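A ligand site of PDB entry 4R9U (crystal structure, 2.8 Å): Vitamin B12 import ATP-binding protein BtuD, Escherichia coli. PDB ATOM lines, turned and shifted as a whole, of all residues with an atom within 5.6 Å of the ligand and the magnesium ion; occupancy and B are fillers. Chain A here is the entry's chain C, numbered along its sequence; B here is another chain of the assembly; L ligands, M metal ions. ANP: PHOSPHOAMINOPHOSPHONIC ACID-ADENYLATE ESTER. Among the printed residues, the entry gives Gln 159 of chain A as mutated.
An oxygen (O1A) of the ligand sits at hydrogen-bond distance from the backbone NH (N) of Ser 40. The backbone NH (N) of Lys 39 is in hydrogen-bond range of an oxygen (O1B) of the ligand, at 2.7 Å. O1B of the ligand lies within salt-bridge range of NZ of Lys 39 (2.7 Å). N of Thr 41 sits at hydrogen-bond distance from O1A of the ligand (2.8 Å). OG1 of Thr 41 is in hydrogen-bond range of O1A of the ligand (2.8 Å). An oxygen (O2') of the ligand is in hydrogen-bond range of the side-chain carboxylate of Glu 131 of chain B (2.8 Å). The side-chain hydroxyl (OG) of Ser 128 of chain B sits at hydrogen-bond distance from an oxygen (O2G) of the ligand (2.8 Å). An oxygen (O1G) of the ligand lies within hydrogen-bond range of a ring nitrogen (NE2) of His 191, at 2.9 Å. An oxygen (O2') of the ligand lies within hydrogen-bond range of the guanidinium group (NH1) of Arg 122 of chain B (3.0 Å). OD1 of Asn 35 sits close to O2G of the ligand (3.0 Å). The backbone NH (N) of Gly 130 of chain B is in hydrogen-bond range of an oxygen (O2G) of the ligand, 3.0 Å away. An oxygen (O1B) of the ligand is in hydrogen-bond range of the backbone NH (N) of Gly 38, 3.2 Å away.
The side-chain carboxylate (OD2) of Asp 158 sits close to the side-chain hydroxyl (OG) of Ser 40 (2.7 Å). The side-chain amide oxygen (OE1) of Gln 159 sits close to the side-chain amide oxygen (OE1) of Gln 80, 3.3 Å away. The side-chain amino group of Lys 39 lies within hydrogen-bond range of the backbone carbonyl oxygen of Pro 34 (3.1 Å). NZ of Lys 39 lies within hydrogen-bond range of O of Gly 33, 2.9 Å away. N of Ser 128 of chain B sits at hydrogen-bond distance from OE1 of Glu 131 of chain B, 2.9 Å away. OG of Ser 128 of chain B is in hydrogen-bond range of N of Gly 130 of chain B (3.0 Å). The backbone carbonyl oxygen of Gln 126 of chain B sits at hydrogen-bond distance from the guanidinium group of Arg 122 of chain B (3.4 Å). OD1 of Asn 35 sits close to O of Ser 163 of chain B, at 3.4 Å.
N3B of the ligand sits close to N of Gly 36, 3.3 Å away. Arg 15 touches the ligand (CB to O4', 3.3 Å). Gln 159 touches the ligand (OE1 to O1G, 3.5 Å). Gln 126 of chain B touches the ligand (CG to N6, 3.5 Å). O of Leu 127 of chain B touches N7 of the ligand, 3.9 Å away. N of Gly 129 of chain B touches O3G of the ligand (3.6 Å). Ser 163 of chain B touches the ligand. Hydrophobic or aromatic side chains that line the ligand: His 191. 18 residues have an atom within 4 Å of the ligand: Arg 15, Asn 35, Gly 36, Gly 38, Lys 39, Ser 40, Thr 41, Gln 80, Gln 159, His 191, Arg 122 of chain B, Gln 126 of chain B, Leu 127 of chain B, Ser 128 of chain B, Gly 129 of chain B, Gly 130 of chain B, Glu 131 of chain B and Ser 163 of chain B.
Merely in contact with the magnesium ion: Gln 159. The nearest printed residue that does not touch the magnesium ion is Asp 158 (4.02 Å).
OG of Ser 40 is bound to the magnesium ion, at 1.9 Å. The magnesium ion is bound by O2B of the ligand. An oxygen (O3G) of the ligand is bound to the magnesium ion, 2.2 Å away. The magnesium ion is bound by NE2 of Gln 80, at 2.4 Å. The magnesium ion has four donor atoms within binding distance. Slightly farther from the magnesium ion lies the side-chain amide oxygen (OE1) of Gln 80 (2.8 Å).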
ATOM      1  N   ARG A  15      -0.222 -18.677  -8.584  1.00  0.00           N
ATOM      2  CA  ARG A  15      -0.548 -19.470  -9.756  1.00  0.00           C
ATOM      3  C   ARG A  15      -1.325 -20.717  -9.351  1.00  0.00           C
ATOM      4  O   ARG A  15      -1.766 -21.483 -10.211  1.00  0.00           O
ATOM      5  CB  ARG A  15       0.723 -19.840 -10.555  1.00  0.00           C
ATOM      6  CG  ARG A  15       1.614 -20.868  -9.906  1.00  0.00           C
ATOM      7  CD  ARG A  15       2.655 -21.385 -10.906  1.00  0.00           C
ATOM      8  NE  ARG A  15       3.988 -20.828 -10.674  1.00  0.00           N
ATOM      9  CZ  ARG A  15       5.110 -21.352 -11.181  1.00  0.00           C
ATOM     10  NH1 ARG A  15       5.055 -22.430 -11.959  1.00  0.00           N
ATOM     11  NH2 ARG A  15       6.279 -20.793 -10.922  1.00  0.00           N
ATOM     12  N   GLY A  33     -10.668 -27.111 -16.751  1.00  0.00           N
ATOM     13  CA  GLY A  33     -10.549 -25.687 -16.524  1.00  0.00           C
ATOM     14  C   GLY A  33      -9.701 -25.013 -17.579  1.00  0.00           C
ATOM     15  O   GLY A  33      -8.937 -25.691 -18.269  1.00  0.00           O
ATOM     16  N   PRO A  34      -9.829 -23.687 -17.713  1.00  0.00           N
ATOM     17  CA  PRO A  34      -9.171 -22.880 -18.746  1.00  0.00           C
ATOM     18  C   PRO A  34      -7.655 -22.851 -18.617  1.00  0.00           C
ATOM     19  O   PRO A  34      -7.112 -23.355 -17.634  1.00  0.00           O
ATOM     20  CB  PRO A  34      -9.739 -21.480 -18.512  1.00  0.00           C
ATOM     21  CG  PRO A  34     -10.150 -21.471 -17.098  1.00  0.00           C
ATOM     22  CD  PRO A  34     -10.631 -22.851 -16.799  1.00  0.00           C
ATOM     23  N   ASN A  35      -6.979 -22.266 -19.603  1.00  0.00           N
ATOM     24  CA  ASN A  35      -5.540 -21.973 -19.522  1.00  0.00           C
ATOM     25  C   ASN A  35      -5.321 -21.076 -18.316  1.00  0.00           C
ATOM     26  O   ASN A  35      -6.025 -20.079 -18.146  1.00  0.00           O
ATOM     27  CB  ASN A  35      -5.047 -21.269 -20.789  1.00  0.00           C
ATOM     28  CG  ASN A  35      -5.270 -22.077 -22.064  1.00  0.00           C
ATOM     29  OD1 ASN A  35      -5.746 -23.219 -22.028  1.00  0.00           O
ATOM     30  ND2 ASN A  35      -5.007 -21.460 -23.202  1.00  0.00           N
ATOM     31  N   GLY A  36      -4.386 -21.430 -17.433  1.00  0.00           N
ATOM     32  CA  GLY A  36      -4.177 -20.590 -16.281  1.00  0.00           C
ATOM     33  C   GLY A  36      -4.993 -21.031 -15.076  1.00  0.00           C
ATOM     34  O   GLY A  36      -5.012 -20.368 -14.036  1.00  0.00           O
ATOM     35  N   ALA A  37      -5.720 -22.128 -15.224  1.00  0.00           N
ATOM     36  CA  ALA A  37      -6.411 -22.694 -14.071  1.00  0.00           C
ATOM     37  C   ALA A  37      -5.400 -23.294 -13.107  1.00  0.00           C
ATOM     38  O   ALA A  37      -5.617 -23.317 -11.903  1.00  0.00           O
ATOM     39  CB  ALA A  37      -7.406 -23.729 -14.501  1.00  0.00           C
ATOM     40  N   GLY A  38      -4.278 -23.773 -13.638  1.00  0.00           N
ATOM     41  CA  GLY A  38      -3.250 -24.377 -12.822  1.00  0.00           C
ATOM     42  C   GLY A  38      -3.392 -25.877 -12.636  1.00  0.00           C
ATOM     43  O   GLY A  38      -3.107 -26.396 -11.572  1.00  0.00           O
ATOM     44  N   LYS A  39      -3.860 -26.565 -13.677  1.00  0.00           N
ATOM     45  CA  LYS A  39      -3.966 -28.023 -13.656  1.00  0.00           C
ATOM     46  C   LYS A  39      -2.572 -28.649 -13.629  1.00  0.00           C
ATOM     47  O   LYS A  39      -2.271 -29.481 -12.782  1.00  0.00           O
ATOM     48  CB  LYS A  39      -4.715 -28.486 -14.896  1.00  0.00           C
ATOM     49  CG  LYS A  39      -6.010 -27.764 -15.072  1.00  0.00           C
ATOM     50  CD  LYS A  39      -6.745 -28.199 -16.340  1.00  0.00           C
ATOM     51  CE  LYS A  39      -6.031 -27.745 -17.604  1.00  0.00           C
ATOM     52  NZ  LYS A  39      -6.184 -26.271 -17.802  1.00  0.00           N
ATOM     53  N   SER A  40      -1.711 -28.186 -14.540  1.00  0.00           N
ATOM     54  CA  SER A  40      -0.371 -28.764 -14.693  1.00  0.00           C
ATOM     55  C   SER A  40       0.404 -28.608 -13.390  1.00  0.00           C
ATOM     56  O   SER A  40       1.158 -29.501 -13.006  1.00  0.00           O
ATOM     57  CB  SER A  40       0.400 -28.097 -15.846  1.00  0.00           C
ATOM     58  OG  SER A  40       0.102 -28.632 -17.141  1.00  0.00           O
ATOM     59  N   THR A  41       0.205 -27.483 -12.705  1.00  0.00           N
ATOM     60  CA  THR A  41       0.907 -27.197 -11.429  1.00  0.00           C
ATOM     61  C   THR A  41       0.487 -28.125 -10.322  1.00  0.00           C
ATOM     62  O   THR A  41       1.319 -28.681  -9.575  1.00  0.00           O
ATOM     63  CB  THR A  41       0.679 -25.765 -10.954  1.00  0.00           C
ATOM     64  OG1 THR A  41       1.133 -24.849 -11.946  1.00  0.00           O
ATOM     65  CG2 THR A  41       1.465 -25.495  -9.671  1.00  0.00           C
ATOM     66  N   LEU A  42      -0.821 -28.257 -10.191  1.00  0.00           N
ATOM     67  CA  LEU A  42      -1.414 -29.138  -9.207  1.00  0.00           C
ATOM     68  C   LEU A  42      -1.003 -30.581  -9.459  1.00  0.00           C
ATOM     69  O   LEU A  42      -0.633 -31.294  -8.538  1.00  0.00           O
ATOM     70  CB  LEU A  42      -2.931 -29.006  -9.218  1.00  0.00           C
ATOM     71  CG  LEU A  42      -3.641 -30.096  -8.434  1.00  0.00           C
ATOM     72  CD1 LEU A  42      -3.243 -30.113  -6.950  1.00  0.00           C
ATOM     73  CD2 LEU A  42      -5.171 -29.952  -8.600  1.00  0.00           C
ATOM     74  N   GLN A  80       3.393 -32.587 -19.144  1.00  0.00           N
ATOM     75  CA  GLN A  80       2.561 -32.115 -20.244  1.00  0.00           C
ATOM     76  C   GLN A  80       3.271 -32.210 -21.600  1.00  0.00           C
ATOM     77  O   GLN A  80       2.695 -32.743 -22.546  1.00  0.00           O
ATOM     78  CB  GLN A  80       2.155 -30.679 -19.972  1.00  0.00           C
ATOM     79  CG  GLN A  80       1.518 -29.939 -21.123  1.00  0.00           C
ATOM     80  CD  GLN A  80       0.498 -28.915 -20.633  1.00  0.00           C
ATOM     81  OE1 GLN A  80      -0.701 -29.039 -20.889  1.00  0.00           O
ATOM     82  NE2 GLN A  80       0.973 -27.934 -19.895  1.00  0.00           N
ATOM     83  N   ASP A 158      -0.900 -35.608 -17.627  1.00  0.00           N
ATOM     84  CA  ASP A 158      -1.160 -34.224 -18.007  1.00  0.00           C
ATOM     85  C   ASP A 158      -1.575 -34.069 -19.456  1.00  0.00           C
ATOM     86  O   ASP A 158      -0.730 -34.000 -20.336  1.00  0.00           O
ATOM     87  CB  ASP A 158       0.047 -33.362 -17.696  1.00  0.00           C
ATOM     88  CG  ASP A 158      -0.331 -31.955 -17.274  1.00  0.00           C
ATOM     89  OD1 ASP A 158      -1.522 -31.579 -17.382  1.00  0.00           O
ATOM     90  OD2 ASP A 158       0.576 -31.243 -16.812  1.00  0.00           O
ATOM     91  N   GLN A 159      -2.881 -34.081 -19.720  1.00  0.00           N
ATOM     92  CA  GLN A 159      -3.370 -33.876 -21.076  1.00  0.00           C
ATOM     93  C   GLN A 159      -2.732 -34.865 -21.998  1.00  0.00           C
ATOM     94  O   GLN A 159      -1.934 -34.486 -22.862  1.00  0.00           O
ATOM     95  CB  GLN A 159      -3.096 -32.463 -21.558  1.00  0.00           C
ATOM     96  CG  GLN A 159      -4.326 -31.637 -21.438  1.00  0.00           C
ATOM     97  CD  GLN A 159      -4.035 -30.181 -21.208  1.00  0.00           C
ATOM     98  OE1 GLN A 159      -3.776 -29.754 -20.068  1.00  0.00           O
ATOM     99  NE2 GLN A 159      -4.070 -29.408 -22.287  1.00  0.00           N
ATOM    100  N   HIS A 191      -9.198 -31.086 -21.839  1.00  0.00           N
ATOM    101  CA  HIS A 191      -9.839 -29.895 -22.334  1.00  0.00           C
ATOM    102  C   HIS A 191     -11.086 -30.200 -23.150  1.00  0.00           C
ATOM    103  O   HIS A 191     -11.736 -29.280 -23.628  1.00  0.00           O
ATOM    104  CB  HIS A 191      -8.869 -29.105 -23.157  1.00  0.00           C
ATOM    105  CG  HIS A 191      -8.091 -28.128 -22.341  1.00  0.00           C
ATOM    106  ND1 HIS A 191      -8.642 -26.973 -21.843  1.00  0.00           N
ATOM    107  CD2 HIS A 191      -6.786 -28.131 -21.948  1.00  0.00           C
ATOM    108  CE1 HIS A 191      -7.730 -26.296 -21.181  1.00  0.00           C
ATOM    109  NE2 HIS A 191      -6.592 -26.980 -21.221  1.00  0.00           N
ATOM    110  N   ARG B 122       5.865 -10.895 -19.651  1.00  0.00           N
ATOM    111  CA  ARG B 122       6.372 -12.120 -19.062  1.00  0.00           C
ATOM    112  C   ARG B 122       7.308 -12.853 -20.023  1.00  0.00           C
ATOM    113  O   ARG B 122       7.171 -12.733 -21.244  1.00  0.00           O
ATOM    114  CB  ARG B 122       5.188 -12.983 -18.660  1.00  0.00           C
ATOM    115  CG  ARG B 122       5.524 -14.033 -17.670  1.00  0.00           C
ATOM    116  CD  ARG B 122       4.636 -13.880 -16.465  1.00  0.00           C
ATOM    117  NE  ARG B 122       3.228 -13.939 -16.829  1.00  0.00           N
ATOM    118  CZ  ARG B 122       2.449 -15.010 -16.631  1.00  0.00           C
ATOM    119  NH1 ARG B 122       2.964 -16.094 -16.070  1.00  0.00           N
ATOM    120  NH2 ARG B 122       1.173 -14.993 -16.988  1.00  0.00           N
ATOM    121  N   ASN B 125       9.435 -18.772 -21.519  1.00  0.00           N
ATOM    122  CA  ASN B 125       9.693 -20.061 -20.861  1.00  0.00           C
ATOM    123  C   ASN B 125       9.015 -20.129 -19.504  1.00  0.00           C
ATOM    124  O   ASN B 125       9.259 -21.042 -18.711  1.00  0.00           O
ATOM    125  CB  ASN B 125      11.206 -20.329 -20.682  1.00  0.00           C
ATOM    126  CG  ASN B 125      11.918 -19.217 -19.923  1.00  0.00           C
ATOM    127  OD1 ASN B 125      11.710 -18.027 -20.200  1.00  0.00           O
ATOM    128  ND2 ASN B 125      12.725 -19.595 -18.940  1.00  0.00           N
ATOM    129  N   GLN B 126       8.161 -19.154 -19.225  1.00  0.00           N
ATOM    130  CA  GLN B 126       7.457 -19.070 -17.965  1.00  0.00           C
ATOM    131  C   GLN B 126       5.961 -18.940 -18.178  1.00  0.00           C
ATOM    132  O   GLN B 126       5.297 -18.100 -17.557  1.00  0.00           O
ATOM    133  CB  GLN B 126       7.977 -17.888 -17.148  1.00  0.00           C
ATOM    134  CG  GLN B 126       9.300 -18.130 -16.454  1.00  0.00           C
ATOM    135  CD  GLN B 126       9.706 -16.949 -15.602  1.00  0.00           C
ATOM    136  OE1 GLN B 126       9.099 -15.877 -15.683  1.00  0.00           O
ATOM    137  NE2 GLN B 126      10.749 -17.114 -14.794  1.00  0.00           N
ATOM    138  N   LEU B 127       5.427 -19.747 -19.100  1.00  0.00           N
ATOM    139  CA  LEU B 127       3.999 -19.744 -19.344  1.00  0.00           C
ATOM    140  C   LEU B 127       3.379 -21.133 -19.224  1.00  0.00           C
ATOM    141  O   LEU B 127       4.075 -22.140 -19.161  1.00  0.00           O
ATOM    142  CB  LEU B 127       3.689 -19.194 -20.728  1.00  0.00           C
ATOM    143  CG  LEU B 127       4.217 -17.794 -21.019  1.00  0.00           C
ATOM    144  CD1 LEU B 127       4.007 -17.508 -22.487  1.00  0.00           C
ATOM    145  CD2 LEU B 127       3.498 -16.803 -20.146  1.00  0.00           C
ATOM    146  N   SER B 128       2.046 -21.179 -19.167  1.00  0.00           N
ATOM    147  CA  SER B 128       1.345 -22.443 -19.284  1.00  0.00           C
ATOM    148  C   SER B 128       1.556 -22.989 -20.683  1.00  0.00           C
ATOM    149  O   SER B 128       2.093 -22.303 -21.551  1.00  0.00           O
ATOM    150  CB  SER B 128      -0.142 -22.280 -18.987  1.00  0.00           C
ATOM    151  OG  SER B 128      -0.946 -22.702 -20.078  1.00  0.00           O
ATOM    152  N   GLY B 129       1.161 -24.238 -20.905  1.00  0.00           N
ATOM    153  CA  GLY B 129       1.327 -24.846 -22.220  1.00  0.00           C
ATOM    154  C   GLY B 129       0.444 -24.094 -23.195  1.00  0.00           C
ATOM    155  O   GLY B 129       0.881 -23.642 -24.272  1.00  0.00           O
ATOM    156  N   GLY B 130      -0.804 -23.896 -22.789  1.00  0.00           N
ATOM    157  CA  GLY B 130      -1.746 -23.167 -23.604  1.00  0.00           C
ATOM    158  C   GLY B 130      -1.316 -21.735 -23.897  1.00  0.00           C
ATOM    159  O   GLY B 130      -1.416 -21.279 -25.038  1.00  0.00           O
ATOM    160  N   GLU B 131      -0.845 -21.038 -22.873  1.00  0.00           N
ATOM    161  CA  GLU B 131      -0.411 -19.657 -23.032  1.00  0.00           C
ATOM    162  C   GLU B 131       0.691 -19.476 -24.079  1.00  0.00           C
ATOM    163  O   GLU B 131       0.575 -18.657 -24.989  1.00  0.00           O
ATOM    164  CB  GLU B 131       0.022 -19.093 -21.674  1.00  0.00           C
ATOM    165  CG  GLU B 131      -1.158 -19.064 -20.680  1.00  0.00           C
ATOM    166  CD  GLU B 131      -0.787 -18.554 -19.293  1.00  0.00           C
ATOM    167  OE1 GLU B 131       0.281 -18.947 -18.782  1.00  0.00           O
ATOM    168  OE2 GLU B 131      -1.582 -17.800 -18.683  1.00  0.00           O
ATOM    169  N   SER B 163      -4.160 -27.946 -26.686  1.00  0.00           N
ATOM    170  CA  SER B 163      -3.765 -27.335 -25.402  1.00  0.00           C
ATOM    171  C   SER B 163      -4.443 -25.972 -25.127  1.00  0.00           C
ATOM    172  O   SER B 163      -4.192 -25.345 -24.102  1.00  0.00           O
ATOM    173  CB  SER B 163      -2.242 -27.171 -25.292  1.00  0.00           C
ATOM    174  OG  SER B 163      -1.824 -25.948 -25.868  1.00  0.00           O
HETATM  175  PG  ANP L   1      -3.066 -25.279 -19.694  1.00  0.00           P
HETATM  176  O1G ANP L   1      -4.178 -26.261 -19.866  1.00  0.00           O
HETATM  177  O2G ANP L   1      -3.145 -24.271 -20.887  1.00  0.00           O
HETATM  178  O3G ANP L   1      -1.703 -26.094 -19.691  1.00  0.00           O
HETATM  179  PB  ANP L   1      -2.734 -25.220 -16.914  1.00  0.00           P
HETATM  180  O1B ANP L   1      -4.005 -25.634 -16.260  1.00  0.00           O
HETATM  181  O2B ANP L   1      -1.951 -26.483 -17.368  1.00  0.00           O
HETATM  182  N3B ANP L   1      -3.179 -24.341 -18.277  1.00  0.00           N
HETATM  183  PA  ANP L   1      -0.420 -24.423 -15.537  1.00  0.00           P
HETATM  184  O1A ANP L   1      -0.278 -25.329 -14.359  1.00  0.00           O
HETATM  185  O2A ANP L   1       0.315 -24.829 -16.822  1.00  0.00           O
HETATM  186  O3A ANP L   1      -1.955 -24.293 -15.918  1.00  0.00           O
HETATM  187  O5' ANP L   1      -0.067 -22.953 -14.991  1.00  0.00           O
HETATM  188  C5' ANP L   1      -1.072 -22.153 -14.282  1.00  0.00           C
HETATM  189  C4' ANP L   1      -0.596 -20.735 -14.060  1.00  0.00           C
HETATM  190  O4' ANP L   1       0.815 -20.739 -13.751  1.00  0.00           O
HETATM  191  C3' ANP L   1      -0.785 -19.782 -15.245  1.00  0.00           C
HETATM  192  O3' ANP L   1      -1.452 -18.583 -14.882  1.00  0.00           O
HETATM  193  C2' ANP L   1       0.642 -19.479 -15.722  1.00  0.00           C
HETATM  194  O2' ANP L   1       0.790 -18.128 -16.167  1.00  0.00           O
HETATM  195  C1' ANP L   1       1.468 -19.705 -14.449  1.00  0.00           C
HETATM  196  N9  ANP L   1       2.840 -20.131 -14.688  1.00  0.00           N
HETATM  197  C8  ANP L   1       3.248 -21.267 -15.329  1.00  0.00           C
HETATM  198  N7  ANP L   1       4.544 -21.416 -15.380  1.00  0.00           N
HETATM  199  C5  ANP L   1       5.031 -20.304 -14.720  1.00  0.00           C
HETATM  200  C6  ANP L   1       6.345 -19.870 -14.430  1.00  0.00           C
HETATM  201  N6  ANP L   1       7.449 -20.533 -14.796  1.00  0.00           N
HETATM  202  N1  ANP L   1       6.485 -18.714 -13.744  1.00  0.00           N
HETATM  203  C2  ANP L   1       5.382 -18.047 -13.386  1.00  0.00           C
HETATM  204  N3  ANP L   1       4.102 -18.353 -13.592  1.00  0.00           N
HETATM  205  C4  ANP L   1       4.000 -19.503 -14.268  1.00  0.00           C
HETATM  206 MG    MG M   1      -0.915 -27.742 -18.435  1.00  0.00          MG
